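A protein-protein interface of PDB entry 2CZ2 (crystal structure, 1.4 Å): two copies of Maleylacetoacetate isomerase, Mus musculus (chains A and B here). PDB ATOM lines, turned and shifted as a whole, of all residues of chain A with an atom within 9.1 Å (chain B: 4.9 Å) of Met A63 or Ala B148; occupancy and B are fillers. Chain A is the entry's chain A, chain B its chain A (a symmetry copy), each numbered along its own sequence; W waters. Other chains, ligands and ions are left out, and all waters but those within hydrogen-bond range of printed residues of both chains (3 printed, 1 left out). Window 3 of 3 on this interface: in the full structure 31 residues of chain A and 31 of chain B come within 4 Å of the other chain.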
ATOM      1  N   LEU A  45     -33.455  29.197 -13.300  1.00  0.00           N
ATOM      2  CA  LEU A  45     -32.944  27.833 -13.417  1.00  0.00           C
ATOM      3  C   LEU A  45     -33.815  26.905 -14.217  1.00  0.00           C
ATOM      4  O   LEU A  45     -33.388  25.807 -14.507  1.00  0.00           O
ATOM      5  CB  LEU A  45     -32.699  27.247 -12.015  1.00  0.00           C
ATOM      6  CG  LEU A  45     -31.691  27.959 -11.120  1.00  0.00           C
ATOM      7  CD1 LEU A  45     -31.572  27.184  -9.809  1.00  0.00           C
ATOM      8  CD2 LEU A  45     -30.296  28.104 -11.776  1.00  0.00           C
ATOM      9  N   GLN A  52     -28.514  28.918 -16.300  1.00  0.00           N
ATOM     10  CA  GLN A  52     -27.256  28.426 -15.758  1.00  0.00           C
ATOM     11  C   GLN A  52     -26.432  27.681 -16.820  1.00  0.00           C
ATOM     12  O   GLN A  52     -25.267  27.443 -16.625  1.00  0.00           O
ATOM     13  CB  GLN A  52     -27.508  27.538 -14.512  1.00  0.00           C
ATOM     14  CG  GLN A  52     -28.176  26.171 -14.769  1.00  0.00           C
ATOM     15  CD  GLN A  52     -29.703  26.199 -14.750  1.00  0.00           C
ATOM     16  OE1 GLN A  52     -30.309  27.207 -15.150  1.00  0.00           O
ATOM     17  NE2 GLN A  52     -30.332  25.082 -14.337  1.00  0.00           N
ATOM     18  N   PHE A  53     -27.047  27.325 -17.937  1.00  0.00           N
ATOM     19  CA  PHE A  53     -26.332  26.666 -19.018  1.00  0.00           C
ATOM     20  C   PHE A  53     -25.809  27.617 -20.085  1.00  0.00           C
ATOM     21  O   PHE A  53     -25.115  27.167 -21.006  1.00  0.00           O
ATOM     22  CB  PHE A  53     -27.228  25.590 -19.630  1.00  0.00           C
ATOM     23  CG  PHE A  53     -27.573  24.507 -18.659  1.00  0.00           C
ATOM     24  CD1 PHE A  53     -28.835  24.441 -18.112  1.00  0.00           C
ATOM     25  CD2 PHE A  53     -26.617  23.565 -18.266  1.00  0.00           C
ATOM     26  CE1 PHE A  53     -29.178  23.443 -17.203  1.00  0.00           C
ATOM     27  CE2 PHE A  53     -26.936  22.557 -17.340  1.00  0.00           C
ATOM     28  CZ  PHE A  53     -28.227  22.507 -16.800  1.00  0.00           C
ATOM     29  N   PHE A  57     -22.898  32.361 -18.182  1.00  0.00           N
ATOM     30  CA  PHE A  57     -22.941  31.889 -16.804  1.00  0.00           C
ATOM     31  C   PHE A  57     -21.919  30.762 -16.570  1.00  0.00           C
ATOM     32  O   PHE A  57     -21.319  30.684 -15.502  1.00  0.00           O
ATOM     33  CB  PHE A  57     -24.351  31.453 -16.349  1.00  0.00           C
ATOM     34  CG  PHE A  57     -24.421  31.215 -14.885  1.00  0.00           C
ATOM     35  CD1 PHE A  57     -24.407  32.291 -14.007  1.00  0.00           C
ATOM     36  CD2 PHE A  57     -24.390  29.927 -14.362  1.00  0.00           C
ATOM     37  CE1 PHE A  57     -24.414  32.097 -12.655  1.00  0.00           C
ATOM     38  CE2 PHE A  57     -24.367  29.734 -12.978  1.00  0.00           C
ATOM     39  CZ  PHE A  57     -24.387  30.804 -12.133  1.00  0.00           C
ATOM     40  N   GLN A  58     -21.717  29.902 -17.563  1.00  0.00           N
ATOM     41  CA  GLN A  58     -20.689  28.856 -17.483  1.00  0.00           C
ATOM     42  C   GLN A  58     -19.270  29.408 -17.250  1.00  0.00           C
ATOM     43  O   GLN A  58     -18.459  28.745 -16.622  1.00  0.00           O
ATOM     44  CB  GLN A  58     -20.692  27.995 -18.746  1.00  0.00           C
ATOM     45  CG  GLN A  58     -21.872  27.059 -18.891  1.00  0.00           C
ATOM     46  CD  GLN A  58     -21.614  26.032 -19.965  1.00  0.00           C
ATOM     47  OE1 GLN A  58     -20.563  25.392 -19.955  1.00  0.00           O
ATOM     48  NE2 GLN A  58     -22.546  25.883 -20.914  1.00  0.00           N
ATOM     49  N   THR A  59     -18.959  30.608 -17.747  1.00  0.00           N
ATOM     50  CA  THR A  59     -17.649  31.207 -17.485  1.00  0.00           C
ATOM     51  C   THR A  59     -17.561  31.722 -16.048  1.00  0.00           C
ATOM     52  O   THR A  59     -16.485  31.743 -15.454  1.00  0.00           O
ATOM     53  CB  THR A  59     -17.354  32.349 -18.472  1.00  0.00           C
ATOM     54  OG1 THR A  59     -18.260  33.428 -18.230  1.00  0.00           O
ATOM     55  CG2 THR A  59     -17.639  31.931 -19.879  1.00  0.00           C
ATOM     56  N   LEU A  60     -18.705  32.117 -15.491  1.00  0.00           N
ATOM     57  CA  LEU A  60     -18.834  32.534 -14.102  1.00  0.00           C
ATOM     58  C   LEU A  60     -18.697  31.336 -13.155  1.00  0.00           C
ATOM     59  O   LEU A  60     -17.924  31.369 -12.181  1.00  0.00           O
ATOM     60  CB  LEU A  60     -20.197  33.188 -13.926  1.00  0.00           C
ATOM     61  CG  LEU A  60     -20.342  33.924 -12.619  1.00  0.00           C
ATOM     62  CD1 LEU A  60     -19.775  35.322 -12.804  1.00  0.00           C
ATOM     63  CD2 LEU A  60     -21.796  33.973 -12.212  1.00  0.00           C
ATOM     64  N   ASN A  61     -19.437  30.275 -13.465  1.00  0.00           N
ATOM     65  CA  ASN A  61     -19.390  29.038 -12.677  1.00  0.00           C
ATOM     66  C   ASN A  61     -19.502  27.825 -13.584  1.00  0.00           C
ATOM     67  O   ASN A  61     -20.603  27.492 -14.003  1.00  0.00           O
ATOM     68  CB  ASN A  61     -20.542  28.975 -11.667  1.00  0.00           C
ATOM     69  CG  ASN A  61     -20.464  27.710 -10.793  1.00  0.00           C
ATOM     70  OD1 ASN A  61     -19.467  26.967 -10.850  1.00  0.00           O
ATOM     71  ND2 ASN A  61     -21.487  27.473  -9.973  1.00  0.00           N
ATOM     72  N   PRO A  62     -18.381  27.172 -13.904  1.00  0.00           N
ATOM     73  CA  PRO A  62     -18.391  25.987 -14.762  1.00  0.00           C
ATOM     74  C   PRO A  62     -19.276  24.871 -14.229  1.00  0.00           C
ATOM     75  O   PRO A  62     -19.631  23.984 -14.982  1.00  0.00           O
ATOM     76  CB  PRO A  62     -16.927  25.567 -14.759  1.00  0.00           C
ATOM     77  CG  PRO A  62     -16.178  26.818 -14.526  1.00  0.00           C
ATOM     78  CD  PRO A  62     -17.008  27.565 -13.537  1.00  0.00           C
ATOM     79  N   MET A  63     -19.598  24.880 -12.940  1.00  0.00           N
ATOM     80  CA  MET A  63     -20.493  23.881 -12.392  1.00  0.00           C
ATOM     81  C   MET A  63     -21.990  24.112 -12.722  1.00  0.00           C
ATOM     82  O   MET A  63     -22.830  23.266 -12.415  1.00  0.00           O
ATOM     83  CB  MET A  63     -20.291  23.842 -10.884  1.00  0.00           C
ATOM     84  CG  MET A  63     -20.614  22.584 -10.259  1.00  0.00           C
ATOM     85  SD  MET A  63     -19.662  20.919 -10.842  1.00  0.00           S
ATOM     86  CE  MET A  63     -20.521  20.029  -9.394  1.00  0.00           C
ATOM     87  N   LYS A  64     -22.304  25.281 -13.275  1.00  0.00           N
ATOM     88  CA  LYS A  64     -23.632  25.604 -13.801  1.00  0.00           C
ATOM     89  C   LYS A  64     -24.666  25.568 -12.655  1.00  0.00           C
ATOM     90  O   LYS A  64     -25.768  25.057 -12.789  1.00  0.00           O
ATOM     91  CB  LYS A  64     -24.011  24.638 -14.918  1.00  0.00           C
ATOM     92  CG  LYS A  64     -23.037  24.697 -16.098  1.00  0.00           C
ATOM     93  CD  LYS A  64     -23.184  23.501 -17.001  1.00  0.00           C
ATOM     94  CE  LYS A  64     -21.835  22.861 -17.289  1.00  0.00           C
ATOM     95  NZ  LYS A  64     -21.965  21.438 -17.746  1.00  0.00           N
ATOM     96  N   GLN A  65     -24.297  26.187 -11.537  1.00  0.00           N
ATOM     97  CA  GLN A  65     -25.171  26.269 -10.372  1.00  0.00           C
ATOM     98  C   GLN A  65     -25.132  27.670  -9.782  1.00  0.00           C
ATOM     99  O   GLN A  65     -24.134  28.397  -9.924  1.00  0.00           O
ATOM    100  CB  GLN A  65     -24.722  25.267  -9.310  1.00  0.00           C
ATOM    101  CG  GLN A  65     -24.874  23.820  -9.752  1.00  0.00           C
ATOM    102  CD  GLN A  65     -24.171  22.837  -8.864  1.00  0.00           C
ATOM    103  OE1 GLN A  65     -23.317  23.211  -8.050  1.00  0.00           O
ATOM    104  NE2 GLN A  65     -24.517  21.551  -9.021  1.00  0.00           N
ATOM    105  N   VAL A  66     -26.196  28.027  -9.059  1.00  0.00           N
ATOM    106  CA  VAL A  66     -26.190  29.187  -8.170  1.00  0.00           C
ATOM    107  C   VAL A  66     -26.129  28.699  -6.743  1.00  0.00           C
ATOM    108  O   VAL A  66     -26.560  27.598  -6.446  1.00  0.00           O
ATOM    109  CB  VAL A  66     -27.428  30.098  -8.346  1.00  0.00           C
ATOM    110  CG1 VAL A  66     -27.403  30.799  -9.713  1.00  0.00           C
ATOM    111  CG2 VAL A  66     -28.690  29.326  -8.163  1.00  0.00           C
ATOM    112  N   PRO A  67     -25.606  29.499  -5.812  1.00  0.00           N
ATOM    113  CA  PRO A  67     -25.150  30.874  -6.007  1.00  0.00           C
ATOM    114  C   PRO A  67     -23.723  31.022  -6.473  1.00  0.00           C
ATOM    115  O   PRO A  67     -22.895  30.135  -6.365  1.00  0.00           O
ATOM    116  CB  PRO A  67     -25.272  31.461  -4.600  1.00  0.00           C
ATOM    117  CG  PRO A  67     -24.987  30.311  -3.714  1.00  0.00           C
ATOM    118  CD  PRO A  67     -25.598  29.137  -4.386  1.00  0.00           C
ATOM    119  N   VAL A  77     -17.845  30.622  -5.730  1.00  0.00           N
ATOM    120  CA  VAL A  77     -18.968  29.709  -5.861  1.00  0.00           C
ATOM    121  C   VAL A  77     -18.934  28.729  -4.678  1.00  0.00           C
ATOM    122  O   VAL A  77     -17.982  28.761  -3.866  1.00  0.00           O
ATOM    123  CB  VAL A  77     -18.973  28.961  -7.209  1.00  0.00           C
ATOM    124  CG1 VAL A  77     -19.012  29.958  -8.384  1.00  0.00           C
ATOM    125  CG2 VAL A  77     -17.797  28.079  -7.359  1.00  0.00           C
ATOM    126  N   GLN A  78     -20.036  27.994  -4.512  1.00  0.00           N
ATOM    127  CA  GLN A  78     -20.287  27.064  -3.411  1.00  0.00           C
ATOM    128  C   GLN A  78     -20.758  27.835  -2.172  1.00  0.00           C
ATOM    129  O   GLN A  78     -20.004  28.569  -1.542  1.00  0.00           O
ATOM    130  CB  GLN A  78     -19.095  26.171  -3.112  1.00  0.00           C
ATOM    131  CG  GLN A  78     -18.805  25.160  -4.206  1.00  0.00           C
ATOM    132  CD  GLN A  78     -19.810  24.032  -4.215  1.00  0.00           C
ATOM    133  OE1 GLN A  78     -20.501  23.762  -3.201  1.00  0.00           O
ATOM    134  NE2 GLN A  78     -19.898  23.345  -5.350  1.00  0.00           N
ATOM    135  N   PRO A 119     -27.871  17.997  -2.505  1.00  0.00           N
ATOM    136  CA  PRO A 119     -27.417  17.592  -3.839  1.00  0.00           C
ATOM    137  C   PRO A 119     -28.282  16.500  -4.462  1.00  0.00           C
ATOM    138  O   PRO A 119     -28.379  16.450  -5.683  1.00  0.00           O
ATOM    139  CB  PRO A 119     -25.983  17.130  -3.603  1.00  0.00           C
ATOM    140  CG  PRO A 119     -25.571  17.844  -2.365  1.00  0.00           C
ATOM    141  CD  PRO A 119     -26.803  17.876  -1.495  1.00  0.00           C
ATOM    142  N   ASN A 122     -31.453  18.137  -5.990  1.00  0.00           N
ATOM    143  CA  ASN A 122     -31.191  19.242  -6.889  1.00  0.00           C
ATOM    144  C   ASN A 122     -31.876  19.001  -8.238  1.00  0.00           C
ATOM    145  O   ASN A 122     -32.086  17.850  -8.649  1.00  0.00           O
ATOM    146  CB  ASN A 122     -29.680  19.399  -7.051  1.00  0.00           C
ATOM    147  CG  ASN A 122     -29.282  20.588  -7.904  1.00  0.00           C
ATOM    148  OD1 ASN A 122     -29.900  21.673  -7.839  1.00  0.00           O
ATOM    149  ND2 ASN A 122     -28.214  20.420  -8.669  1.00  0.00           N
ATOM    150  N   SER A 124     -30.985  19.280 -11.440  1.00  0.00           N
ATOM    151  CA  SER A 124     -30.319  18.451 -12.435  1.00  0.00           C
ATOM    152  C   SER A 124     -30.373  16.956 -12.092  1.00  0.00           C
ATOM    153  O   SER A 124     -30.437  16.126 -12.987  1.00  0.00           O
ATOM    154  CB  SER A 124     -28.865  18.853 -12.644  1.00  0.00           C
ATOM    155  OG  SER A 124     -28.114  18.711 -11.453  1.00  0.00           O
ATOM    156  N   LEU B 112     -17.070  21.406  -4.323  1.00  0.00           N
ATOM    157  CA  LEU B 112     -17.436  20.925  -5.627  1.00  0.00           C
ATOM    158  C   LEU B 112     -17.358  19.388  -5.597  1.00  0.00           C
ATOM    159  O   LEU B 112     -18.265  18.681  -6.019  1.00  0.00           O
ATOM    160  CB  LEU B 112     -16.494  21.504  -6.700  1.00  0.00           C
ATOM    161  CG  LEU B 112     -16.800  21.205  -8.156  1.00  0.00           C
ATOM    162  CD1 LEU B 112     -16.196  22.257  -9.087  1.00  0.00           C
ATOM    163  CD2 LEU B 112     -16.293  19.814  -8.557  1.00  0.00           C
ATOM    164  N   GLY B 116     -20.757  18.281  -4.633  1.00  0.00           N
ATOM    165  CA  GLY B 116     -21.249  18.275  -6.019  1.00  0.00           C
ATOM    166  C   GLY B 116     -21.031  16.979  -6.801  1.00  0.00           C
ATOM    167  O   GLY B 116     -21.707  16.757  -7.810  1.00  0.00           O
ATOM    168  N   ILE B 117     -20.109  16.127  -6.355  1.00  0.00           N
ATOM    169  CA  ILE B 117     -19.826  14.866  -7.057  1.00  0.00           C
ATOM    170  C   ILE B 117     -20.090  13.640  -6.172  1.00  0.00           C
ATOM    171  O   ILE B 117     -20.966  12.815  -6.478  1.00  0.00           O
ATOM    172  CB  ILE B 117     -18.350  14.820  -7.578  1.00  0.00           C
ATOM    173  CG1 ILE B 117     -18.059  15.993  -8.494  1.00  0.00           C
ATOM    174  CG2 ILE B 117     -18.130  13.533  -8.324  1.00  0.00           C
ATOM    175  CD1 ILE B 117     -16.615  16.074  -9.001  1.00  0.00           C
ATOM    176  N   SER B 144     -19.438  15.016 -15.373  1.00  0.00           N
ATOM    177  CA  SER B 144     -19.980  16.367 -15.302  1.00  0.00           C
ATOM    178  C   SER B 144     -19.183  17.234 -14.321  1.00  0.00           C
ATOM    179  O   SER B 144     -18.784  18.371 -14.617  1.00  0.00           O
ATOM    180  CB  SER B 144     -21.458  16.319 -14.912  1.00  0.00           C
ATOM    181  OG  SER B 144     -21.960  17.616 -14.797  1.00  0.00           O
ATOM    182  N   GLY B 145     -18.902  16.667 -13.153  1.00  0.00           N
ATOM    183  CA  GLY B 145     -18.110  17.336 -12.135  1.00  0.00           C
ATOM    184  C   GLY B 145     -16.679  17.609 -12.588  1.00  0.00           C
ATOM    185  O   GLY B 145     -16.146  18.677 -12.347  1.00  0.00           O
ATOM    186  N   PHE B 146     -16.044  16.627 -13.225  1.00  0.00           N
ATOM    187  CA  PHE B 146     -14.673  16.780 -13.658  1.00  0.00           C
ATOM    188  C   PHE B 146     -14.562  17.752 -14.857  1.00  0.00           C
ATOM    189  O   PHE B 146     -13.563  18.439 -15.014  1.00  0.00           O
ATOM    190  CB  PHE B 146     -14.044  15.437 -14.018  1.00  0.00           C
ATOM    191  CG  PHE B 146     -13.534  14.637 -12.836  1.00  0.00           C
ATOM    192  CD1 PHE B 146     -13.855  14.984 -11.538  1.00  0.00           C
ATOM    193  CD2 PHE B 146     -12.751  13.519 -13.054  1.00  0.00           C
ATOM    194  CE1 PHE B 146     -13.359  14.232 -10.470  1.00  0.00           C
ATOM    195  CE2 PHE B 146     -12.285  12.757 -12.017  1.00  0.00           C
ATOM    196  CZ  PHE B 146     -12.569  13.100 -10.733  1.00  0.00           C
ATOM    197  N   ASN B 147     -15.586  17.803 -15.692  1.00  0.00           N
ATOM    198  CA  ASN B 147     -15.618  18.808 -16.763  1.00  0.00           C
ATOM    199  C   ASN B 147     -15.468  20.198 -16.134  1.00  0.00           C
ATOM    200  O   ASN B 147     -14.692  21.028 -16.578  1.00  0.00           O
ATOM    201  CB  ASN B 147     -16.945  18.759 -17.537  1.00  0.00           C
ATOM    202  CG  ASN B 147     -17.063  17.579 -18.493  1.00  0.00           C
ATOM    203  OD1 ASN B 147     -18.140  17.355 -19.081  1.00  0.00           O
ATOM    204  ND2 ASN B 147     -15.982  16.859 -18.695  1.00  0.00           N
ATOM    205  N   ALA B 148     -16.229  20.448 -15.077  1.00  0.00           N
ATOM    206  CA  ALA B 148     -16.183  21.734 -14.396  1.00  0.00           C
ATOM    207  C   ALA B 148     -14.877  21.947 -13.624  1.00  0.00           C
ATOM    208  O   ALA B 148     -14.247  22.995 -13.713  1.00  0.00           O
ATOM    209  CB  ALA B 148     -17.334  21.805 -13.434  1.00  0.00           C
ATOM    210  N   LEU B 149     -14.488  20.945 -12.855  1.00  0.00           N
ATOM    211  CA  LEU B 149     -13.297  21.039 -12.044  1.00  0.00           C
ATOM    212  C   LEU B 149     -12.045  21.288 -12.910  1.00  0.00           C
ATOM    213  O   LEU B 149     -11.202  22.109 -12.581  1.00  0.00           O
ATOM    214  CB  LEU B 149     -13.131  19.770 -11.220  1.00  0.00           C
ATOM    215  CG  LEU B 149     -11.872  19.720 -10.360  1.00  0.00           C
ATOM    216  CD1 LEU B 149     -11.824  20.917  -9.437  1.00  0.00           C
ATOM    217  CD2 LEU B 149     -11.840  18.428  -9.523  1.00  0.00           C
ATOM    218  N   GLU B 150     -11.928  20.571 -14.019  1.00  0.00           N
ATOM    219  CA  GLU B 150     -10.768  20.702 -14.910  1.00  0.00           C
ATOM    220  C   GLU B 150     -10.658  22.126 -15.455  1.00  0.00           C
ATOM    221  O   GLU B 150      -9.563  22.692 -15.525  1.00  0.00           O
ATOM    222  CB  GLU B 150     -10.885  19.712 -16.045  1.00  0.00           C
ATOM    223  CG  GLU B 150      -9.741  19.734 -17.050  1.00  0.00           C
ATOM    224  CD  GLU B 150      -8.440  19.122 -16.550  1.00  0.00           C
ATOM    225  OE1 GLU B 150      -8.380  18.498 -15.469  1.00  0.00           O
ATOM    226  OE2 GLU B 150      -7.444  19.267 -17.265  1.00  0.00           O
ATOM    227  N   LYS B 151     -11.799  22.730 -15.775  1.00  0.00           N
ATOM    228  CA  LYS B 151     -11.822  24.141 -16.178  1.00  0.00           C
ATOM    229  C   LYS B 151     -11.387  25.072 -15.036  1.00  0.00           C
ATOM    230  O   LYS B 151     -10.559  25.940 -15.243  1.00  0.00           O
ATOM    231  CB  LYS B 151     -13.204  24.534 -16.689  1.00  0.00           C
ATOM    232  CG  LYS B 151     -13.594  23.836 -17.970  1.00  0.00           C
ATOM    233  CD  LYS B 151     -14.883  24.418 -18.519  1.00  0.00           C
ATOM    234  CE  LYS B 151     -15.637  23.436 -19.386  1.00  0.00           C
ATOM    235  NZ  LYS B 151     -16.945  23.103 -18.760  1.00  0.00           N
ATOM    236  N   ILE B 152     -11.935  24.895 -13.830  1.00  0.00           N
ATOM    237  CA  ILE B 152     -11.557  25.716 -12.689  1.00  0.00           C
ATOM    238  C   ILE B 152     -10.068  25.634 -12.404  1.00  0.00           C
ATOM    239  O   ILE B 152      -9.425  26.664 -12.164  1.00  0.00           O
ATOM    240  CB  ILE B 152     -12.388  25.316 -11.429  1.00  0.00           C
ATOM    241  CG1 ILE B 152     -13.856  25.747 -11.631  1.00  0.00           C
ATOM    242  CG2 ILE B 152     -11.809  25.941 -10.167  1.00  0.00           C
ATOM    243  CD1 ILE B 152     -14.906  25.005 -10.764  1.00  0.00           C
HETATM  244  O   HOH W   1     -20.513  18.765 -18.594  1.00  0.00           O
HETATM  245  O   HOH W   2     -23.888  18.589  -8.436  1.00  0.00           O
HETATM  246  O   HOH W   3     -20.213  20.330 -15.878  1.00  0.00           O
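The backbone NH of Met A63 lies within hydrogen-bond range of the side-chain amide oxygen of Asn A61, 3.0 Å away. N of Ile B117 lies within hydrogen-bond range of O of Leu B112 (3.2 Å).
Ala B148 touches Pro A62 (CB to O, 3.5 Å). Pro A62 touches Ile B152 (CG to CG1, 3.9 Å). Met A63 touches Leu B112. Met A63 touches Gly B116 (CE to O, 3.8 Å). SD of Met A63 touches CB of Ala B148 (3.6 Å). NE2 of Gln A78 touches CA of Leu B112, 3.5 Å away.
Met A63 touches just these residues of chain B: Leu B112 (3.9 Å), Gly B116 (3.8 Å) and Ala B148 (3.6 Å). Of the printed residues of chain A, Ala B148 touches Pro A62 and Met A63. No residue of chain A comes within 4 Å of Gly B145. Of the printed residues of chain B, Pro A62 touches Ala B148 (3.5 Å) and Ile B152 (3.9 Å). Of the printed residues of chain B, Gln A78 touches Leu B112 (3.5 Å). Of the printed residues of chain A, Leu B112 touches Met A63 and Gln A78. Of the printed residues of chain A, Ile B152 touches Pro A62. Pro A119 touches none of the printed residues of chain B. The nearest residue of chain B that does not touch Met A63 is Gly B145 (4.1 Å). The nearest residue of chain A that does not touch Ala B148 is Lys A64 (6.0 Å). The nearest printed residue of chain B that does not touch Gln A78 is Gly B116 (5.2 Å).
Of the 12 printed residues of chain B, 4 touch a printed residue of chain A.
No position is printed for both chains. Of the 6 pairs that touch across the chains among the printed residues, none has its exchanged pair printed and touching as well.
Water W3 bridges O of Ser B144 (2.7 Å) and NZ of Lys A64 (2.8 Å). Water W1 lies within hydrogen-bond range of the side-chain amide oxygen of Asn B147 and the side-chain amino group of Lys A64. Water W2 lies within hydrogen-bond range of the backbone carbonyl oxygen (O) of Gly B116 (2.9 Å) and the side-chain amide nitrogen (NE2) of Gln A65 (3.1 Å).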
